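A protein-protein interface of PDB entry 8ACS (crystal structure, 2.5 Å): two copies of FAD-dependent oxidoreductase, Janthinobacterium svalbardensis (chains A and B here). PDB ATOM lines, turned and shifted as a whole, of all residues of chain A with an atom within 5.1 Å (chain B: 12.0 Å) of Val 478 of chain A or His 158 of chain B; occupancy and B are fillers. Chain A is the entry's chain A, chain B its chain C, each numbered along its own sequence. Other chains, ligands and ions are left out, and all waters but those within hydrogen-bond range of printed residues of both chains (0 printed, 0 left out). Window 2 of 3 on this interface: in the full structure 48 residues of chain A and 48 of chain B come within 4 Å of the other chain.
Hydrophobic or aromatic side chains of chain A within 4 Å of the printed part of chain B: Phe 252 and Val 478.
Along chain A the printed residues that touch a printed residue of chain B span positions 252 to 478.
Among the printed residues, 8 pairs touch across the chains.
Among the printed residues, no Asp or Glu carboxylate lies within 4 Å of a Lys or Arg side-chain nitrogen of the other chain.
The backbone NH of Ser 387 of chain A sits at hydrogen-bond distance from the backbone carbonyl oxygen of Asp 477 of chain A, 3.1 Å away.
The side-chain hydroxyl (OG) of Ser 387 of chain A sits at hydrogen-bond distance from the backbone carbonyl oxygen (O) of His 232 of chain A (3.2 Å).
No position is printed for both chains.
Of the 8 pairs that touch across the chains among the printed residues, none has its exchanged pair printed and touching as well.
The backbone NH (N) of Phe 252 of chain A is in hydrogen-bond range of the backbone carbonyl oxygen (O) of Met 154 of chain B (2.9 Å).
OG of Ser 387 of chain A lies within hydrogen-bond range of NE2 of His 158 of chain B (3.1 Å).
Among the printed residues, pairs that only touch across the chains: Phe 252 of chain A with Gly 155 of chain B (3.5 Å), Phe 252 of chain A with Ala 156 of chain B (3.8 Å), Phe 252 of chain A with His 158 of chain B (3.1 Å), Asp 388 of chain A with His 158 of chain B (3.5 Å), Val 478 of chain A with Glu 157 of chain B (3.8 Å) and Val 478 of chain A with His 158 of chain B (3.3 Å).
Val 478 of chain A touches two residues of chain B.
His 158 of chain B touches four residues of chain A.
No residue of chain B comes within 4 Å of His 232 of chain A.
Of chain B, only Met 154, Gly 155, Ala 156 and His 158 come within 4 Å of Phe 252 of chain A.
Ser 387 of chain A touches just one residue of chain B: His 158 (3.1 Å).
Of chain B, only His 158 (3.5 Å) comes within 4 Å of Asp 388 of chain A.
No residue of chain B comes within 4 Å of Ile 476 of chain A.
No residue of chain B comes within 4 Å of Asp 477 of chain A.
No residue of chain B comes within 4 Å of Gly 479 of chain A.
Printed residues of chain A within 4 Å of Glu 157 of chain B: Val 478 (3.8 Å).
Of the printed residues of chain A, Ala 156 of chain B touches Phe 252 (3.8 Å).
Printed residues of chain A within 4 Å of Gly 155 of chain B: Phe 252.
Tyr 475 of chain A touches none of the printed residues of chain B.
The nearest residue of chain B that does not touch Val 478 of chain A is Ala 156 of chain B (6.2 Å).
The nearest residue of chain A that does not touch His 158 of chain B is Gly 479 of chain A (4.6 Å).
The nearest printed residue of chain A that does not touch Gly 155 of chain B is Leu 231 of chain A (7.8 Å).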
ATOM      1  N   LEU A 231       2.221  -4.508 -30.120  1.00  0.00           N
ATOM      2  CA  LEU A 231       3.633  -4.819 -29.933  1.00  0.00           C
ATOM      3  C   LEU A 231       3.804  -5.612 -28.638  1.00  0.00           C
ATOM      4  O   LEU A 231       3.049  -5.432 -27.676  1.00  0.00           O
ATOM      5  CB  LEU A 231       4.465  -3.539 -29.916  1.00  0.00           C
ATOM      6  CG  LEU A 231       4.343  -2.627 -31.147  1.00  0.00           C
ATOM      7  CD1 LEU A 231       5.220  -1.344 -31.075  1.00  0.00           C
ATOM      8  CD2 LEU A 231       4.633  -3.386 -32.430  1.00  0.00           C
ATOM      9  N   HIS A 232       4.749  -6.555 -28.629  1.00  0.00           N
ATOM     10  CA  HIS A 232       4.962  -7.322 -27.411  1.00  0.00           C
ATOM     11  C   HIS A 232       6.203  -6.883 -26.656  1.00  0.00           C
ATOM     12  O   HIS A 232       6.401  -7.346 -25.525  1.00  0.00           O
ATOM     13  CB  HIS A 232       5.011  -8.849 -27.681  1.00  0.00           C
ATOM     14  CG  HIS A 232       5.941  -9.257 -28.781  1.00  0.00           C
ATOM     15  ND1 HIS A 232       7.202  -8.719 -28.938  1.00  0.00           N
ATOM     16  CD2 HIS A 232       5.792 -10.157 -29.778  1.00  0.00           C
ATOM     17  CE1 HIS A 232       7.777  -9.248 -30.002  1.00  0.00           C
ATOM     18  NE2 HIS A 232       6.946 -10.132 -30.520  1.00  0.00           N
ATOM     19  N   PHE A 252       2.338  -0.981 -24.906  1.00  0.00           N
ATOM     20  CA  PHE A 252       2.255  -1.982 -25.964  1.00  0.00           C
ATOM     21  C   PHE A 252       1.313  -1.469 -27.048  1.00  0.00           C
ATOM     22  O   PHE A 252       0.099  -1.413 -26.837  1.00  0.00           O
ATOM     23  CB  PHE A 252       1.771  -3.320 -25.392  1.00  0.00           C
ATOM     24  CG  PHE A 252       2.648  -3.868 -24.327  1.00  0.00           C
ATOM     25  CD1 PHE A 252       3.916  -4.303 -24.627  1.00  0.00           C
ATOM     26  CD2 PHE A 252       2.202  -3.992 -23.029  1.00  0.00           C
ATOM     27  CE1 PHE A 252       4.745  -4.825 -23.633  1.00  0.00           C
ATOM     28  CE2 PHE A 252       3.021  -4.515 -22.040  1.00  0.00           C
ATOM     29  CZ  PHE A 252       4.290  -4.934 -22.341  1.00  0.00           C
ATOM     30  N   SER A 387       5.050 -11.486 -21.463  1.00  0.00           N
ATOM     31  CA  SER A 387       5.373 -10.105 -21.849  1.00  0.00           C
ATOM     32  C   SER A 387       5.755  -9.248 -20.641  1.00  0.00           C
ATOM     33  O   SER A 387       6.740  -8.500 -20.675  1.00  0.00           O
ATOM     34  CB  SER A 387       4.172  -9.496 -22.576  1.00  0.00           C
ATOM     35  OG  SER A 387       4.486  -8.263 -23.192  1.00  0.00           O
ATOM     36  N   ASP A 388       4.958  -9.323 -19.572  1.00  0.00           N
ATOM     37  CA  ASP A 388       5.228  -8.571 -18.344  1.00  0.00           C
ATOM     38  C   ASP A 388       6.581  -8.916 -17.743  1.00  0.00           C
ATOM     39  O   ASP A 388       7.288  -8.037 -17.240  1.00  0.00           O
ATOM     40  CB  ASP A 388       4.105  -8.826 -17.346  1.00  0.00           C
ATOM     41  CG  ASP A 388       2.753  -8.989 -18.049  1.00  0.00           C
ATOM     42  OD1 ASP A 388       2.129  -7.949 -18.404  1.00  0.00           O
ATOM     43  OD2 ASP A 388       2.361 -10.162 -18.310  1.00  0.00           O
ATOM     44  N   TYR A 475       7.775 -17.645 -28.196  1.00  0.00           N
ATOM     45  CA  TYR A 475       6.550 -16.866 -28.237  1.00  0.00           C
ATOM     46  C   TYR A 475       6.449 -16.049 -26.959  1.00  0.00           C
ATOM     47  O   TYR A 475       6.448 -16.615 -25.862  1.00  0.00           O
ATOM     48  CB  TYR A 475       5.337 -17.771 -28.397  1.00  0.00           C
ATOM     49  CG  TYR A 475       4.033 -17.091 -28.074  1.00  0.00           C
ATOM     50  CD1 TYR A 475       3.520 -16.079 -28.873  1.00  0.00           C
ATOM     51  CD2 TYR A 475       3.326 -17.459 -26.952  1.00  0.00           C
ATOM     52  CE1 TYR A 475       2.320 -15.485 -28.562  1.00  0.00           C
ATOM     53  CE2 TYR A 475       2.143 -16.879 -26.634  1.00  0.00           C
ATOM     54  CZ  TYR A 475       1.640 -15.898 -27.425  1.00  0.00           C
ATOM     55  OH  TYR A 475       0.445 -15.343 -27.035  1.00  0.00           O
ATOM     56  N   ILE A 476       6.342 -14.728 -27.109  1.00  0.00           N
ATOM     57  CA  ILE A 476       6.139 -13.812 -25.985  1.00  0.00           C
ATOM     58  C   ILE A 476       4.650 -13.786 -25.653  1.00  0.00           C
ATOM     59  O   ILE A 476       3.831 -13.293 -26.433  1.00  0.00           O
ATOM     60  CB  ILE A 476       6.675 -12.414 -26.311  1.00  0.00           C
ATOM     61  CG1 ILE A 476       8.192 -12.500 -26.498  1.00  0.00           C
ATOM     62  CG2 ILE A 476       6.358 -11.430 -25.205  1.00  0.00           C
ATOM     63  CD1 ILE A 476       8.818 -11.519 -27.443  1.00  0.00           C
ATOM     64  N   ASP A 477       4.298 -14.316 -24.484  1.00  0.00           N
ATOM     65  CA  ASP A 477       2.901 -14.586 -24.166  1.00  0.00           C
ATOM     66  C   ASP A 477       2.185 -13.305 -23.790  1.00  0.00           C
ATOM     67  O   ASP A 477       2.533 -12.671 -22.788  1.00  0.00           O
ATOM     68  CB  ASP A 477       2.753 -15.577 -23.021  1.00  0.00           C
ATOM     69  CG  ASP A 477       1.304 -15.814 -22.673  1.00  0.00           C
ATOM     70  OD1 ASP A 477       0.496 -15.933 -23.612  1.00  0.00           O
ATOM     71  OD2 ASP A 477       0.954 -15.874 -21.481  1.00  0.00           O
ATOM     72  N   VAL A 478       1.162 -12.955 -24.568  1.00  0.00           N
ATOM     73  CA  VAL A 478       0.279 -11.836 -24.265  1.00  0.00           C
ATOM     74  C   VAL A 478      -1.125 -12.317 -23.935  1.00  0.00           C
ATOM     75  O   VAL A 478      -2.046 -11.507 -23.839  1.00  0.00           O
ATOM     76  CB  VAL A 478       0.262 -10.798 -25.405  1.00  0.00           C
ATOM     77  CG1 VAL A 478       1.612 -10.139 -25.529  1.00  0.00           C
ATOM     78  CG2 VAL A 478      -0.109 -11.426 -26.740  1.00  0.00           C
ATOM     79  N   GLY A 479      -1.307 -13.627 -23.758  1.00  0.00           N
ATOM     80  CA  GLY A 479      -2.574 -14.204 -23.344  1.00  0.00           C
ATOM     81  C   GLY A 479      -2.857 -15.609 -23.858  1.00  0.00           C
ATOM     82  O   GLY A 479      -3.671 -16.322 -23.257  1.00  0.00           O
ATOM     83  N   ALA A 480      -2.178 -16.040 -24.936  1.00  0.00           N
ATOM     84  CA  ALA A 480      -2.534 -17.314 -25.551  1.00  0.00           C
ATOM     85  C   ALA A 480      -2.047 -18.515 -24.740  1.00  0.00           C
ATOM     86  O   ALA A 480      -2.732 -19.542 -24.720  1.00  0.00           O
ATOM     87  CB  ALA A 480      -2.003 -17.389 -26.991  1.00  0.00           C
ATOM     88  N   ARG B 152       1.465   5.587 -17.876  1.00  0.00           N
ATOM     89  CA  ARG B 152       1.133   5.237 -19.250  1.00  0.00           C
ATOM     90  C   ARG B 152       0.007   4.211 -19.319  1.00  0.00           C
ATOM     91  O   ARG B 152      -0.021   3.254 -18.520  1.00  0.00           O
ATOM     92  CB  ARG B 152       2.339   4.620 -19.957  1.00  0.00           C
ATOM     93  CG  ARG B 152       3.283   5.564 -20.583  1.00  0.00           C
ATOM     94  CD  ARG B 152       4.549   4.830 -20.926  1.00  0.00           C
ATOM     95  NE  ARG B 152       5.673   5.752 -21.020  1.00  0.00           N
ATOM     96  CZ  ARG B 152       5.900   6.488 -22.095  1.00  0.00           C
ATOM     97  NH1 ARG B 152       5.095   6.432 -23.148  1.00  0.00           N
ATOM     98  NH2 ARG B 152       6.966   7.284 -22.124  1.00  0.00           N
ATOM     99  N   PRO B 153      -0.896   4.340 -20.294  1.00  0.00           N
ATOM    100  CA  PRO B 153      -1.781   3.219 -20.631  1.00  0.00           C
ATOM    101  C   PRO B 153      -0.952   2.004 -21.047  1.00  0.00           C
ATOM    102  O   PRO B 153       0.128   2.142 -21.629  1.00  0.00           O
ATOM    103  CB  PRO B 153      -2.614   3.759 -21.806  1.00  0.00           C
ATOM    104  CG  PRO B 153      -2.247   5.187 -21.962  1.00  0.00           C
ATOM    105  CD  PRO B 153      -0.933   5.399 -21.317  1.00  0.00           C
ATOM    106  N   MET B 154      -1.460   0.800 -20.733  1.00  0.00           N
ATOM    107  CA  MET B 154      -0.793  -0.427 -21.192  1.00  0.00           C
ATOM    108  C   MET B 154      -0.954  -0.635 -22.687  1.00  0.00           C
ATOM    109  O   MET B 154      -0.042  -1.145 -23.344  1.00  0.00           O
ATOM    110  CB  MET B 154      -1.325  -1.649 -20.452  1.00  0.00           C
ATOM    111  CG  MET B 154      -0.961  -1.666 -18.966  1.00  0.00           C
ATOM    112  SD  MET B 154       0.788  -1.374 -18.613  1.00  0.00           S
ATOM    113  CE  MET B 154       1.486  -2.904 -19.229  1.00  0.00           C
ATOM    114  N   GLY B 155      -2.090  -0.241 -23.226  1.00  0.00           N
ATOM    115  CA  GLY B 155      -2.436  -0.357 -24.626  1.00  0.00           C
ATOM    116  C   GLY B 155      -3.132  -1.657 -24.871  1.00  0.00           C
ATOM    117  O   GLY B 155      -4.243  -1.671 -25.396  1.00  0.00           O
ATOM    118  N   ALA B 156      -2.520  -2.758 -24.422  1.00  0.00           N
ATOM    119  CA  ALA B 156      -3.014  -4.115 -24.622  1.00  0.00           C
ATOM    120  C   ALA B 156      -3.394  -4.747 -23.294  1.00  0.00           C
ATOM    121  O   ALA B 156      -2.715  -4.539 -22.280  1.00  0.00           O
ATOM    122  CB  ALA B 156      -1.961  -5.002 -25.298  1.00  0.00           C
ATOM    123  N   GLU B 157      -4.461  -5.543 -23.313  1.00  0.00           N
ATOM    124  CA  GLU B 157      -4.800  -6.414 -22.195  1.00  0.00           C
ATOM    125  C   GLU B 157      -4.028  -7.716 -22.371  1.00  0.00           C
ATOM    126  O   GLU B 157      -4.157  -8.380 -23.407  1.00  0.00           O
ATOM    127  CB  GLU B 157      -6.303  -6.688 -22.130  1.00  0.00           C
ATOM    128  CG  GLU B 157      -7.214  -5.505 -22.475  1.00  0.00           C
ATOM    129  CD  GLU B 157      -7.976  -5.725 -23.778  1.00  0.00           C
ATOM    130  OE1 GLU B 157      -7.325  -5.791 -24.844  1.00  0.00           O
ATOM    131  OE2 GLU B 157      -9.224  -5.854 -23.737  1.00  0.00           O
ATOM    132  N   HIS B 158      -3.215  -8.063 -21.372  1.00  0.00           N
ATOM    133  CA  HIS B 158      -2.322  -9.228 -21.442  1.00  0.00           C
ATOM    134  C   HIS B 158      -2.907 -10.429 -20.680  1.00  0.00           C
ATOM    135  O   HIS B 158      -2.252 -11.026 -19.819  1.00  0.00           O
ATOM    136  CB  HIS B 158      -0.924  -8.870 -20.897  1.00  0.00           C
ATOM    137  CG  HIS B 158      -0.031  -8.177 -21.890  1.00  0.00           C
ATOM    138  ND1 HIS B 158      -0.367  -8.017 -23.219  1.00  0.00           N
ATOM    139  CD2 HIS B 158       1.195  -7.616 -21.746  1.00  0.00           C
ATOM    140  CE1 HIS B 158       0.610  -7.384 -23.850  1.00  0.00           C
ATOM    141  NE2 HIS B 158       1.570  -7.131 -22.979  1.00  0.00           N
ATOM    142  N   SER B 165     -13.010  -5.873 -28.164  1.00  0.00           N
ATOM    143  CA  SER B 165     -13.083  -4.754 -29.108  1.00  0.00           C
ATOM    144  C   SER B 165     -11.724  -4.071 -29.293  1.00  0.00           C
ATOM    145  O   SER B 165     -11.159  -3.562 -28.336  1.00  0.00           O
ATOM    146  CB  SER B 165     -14.113  -3.731 -28.650  1.00  0.00           C
ATOM    147  OG  SER B 165     -14.246  -2.716 -29.626  1.00  0.00           O
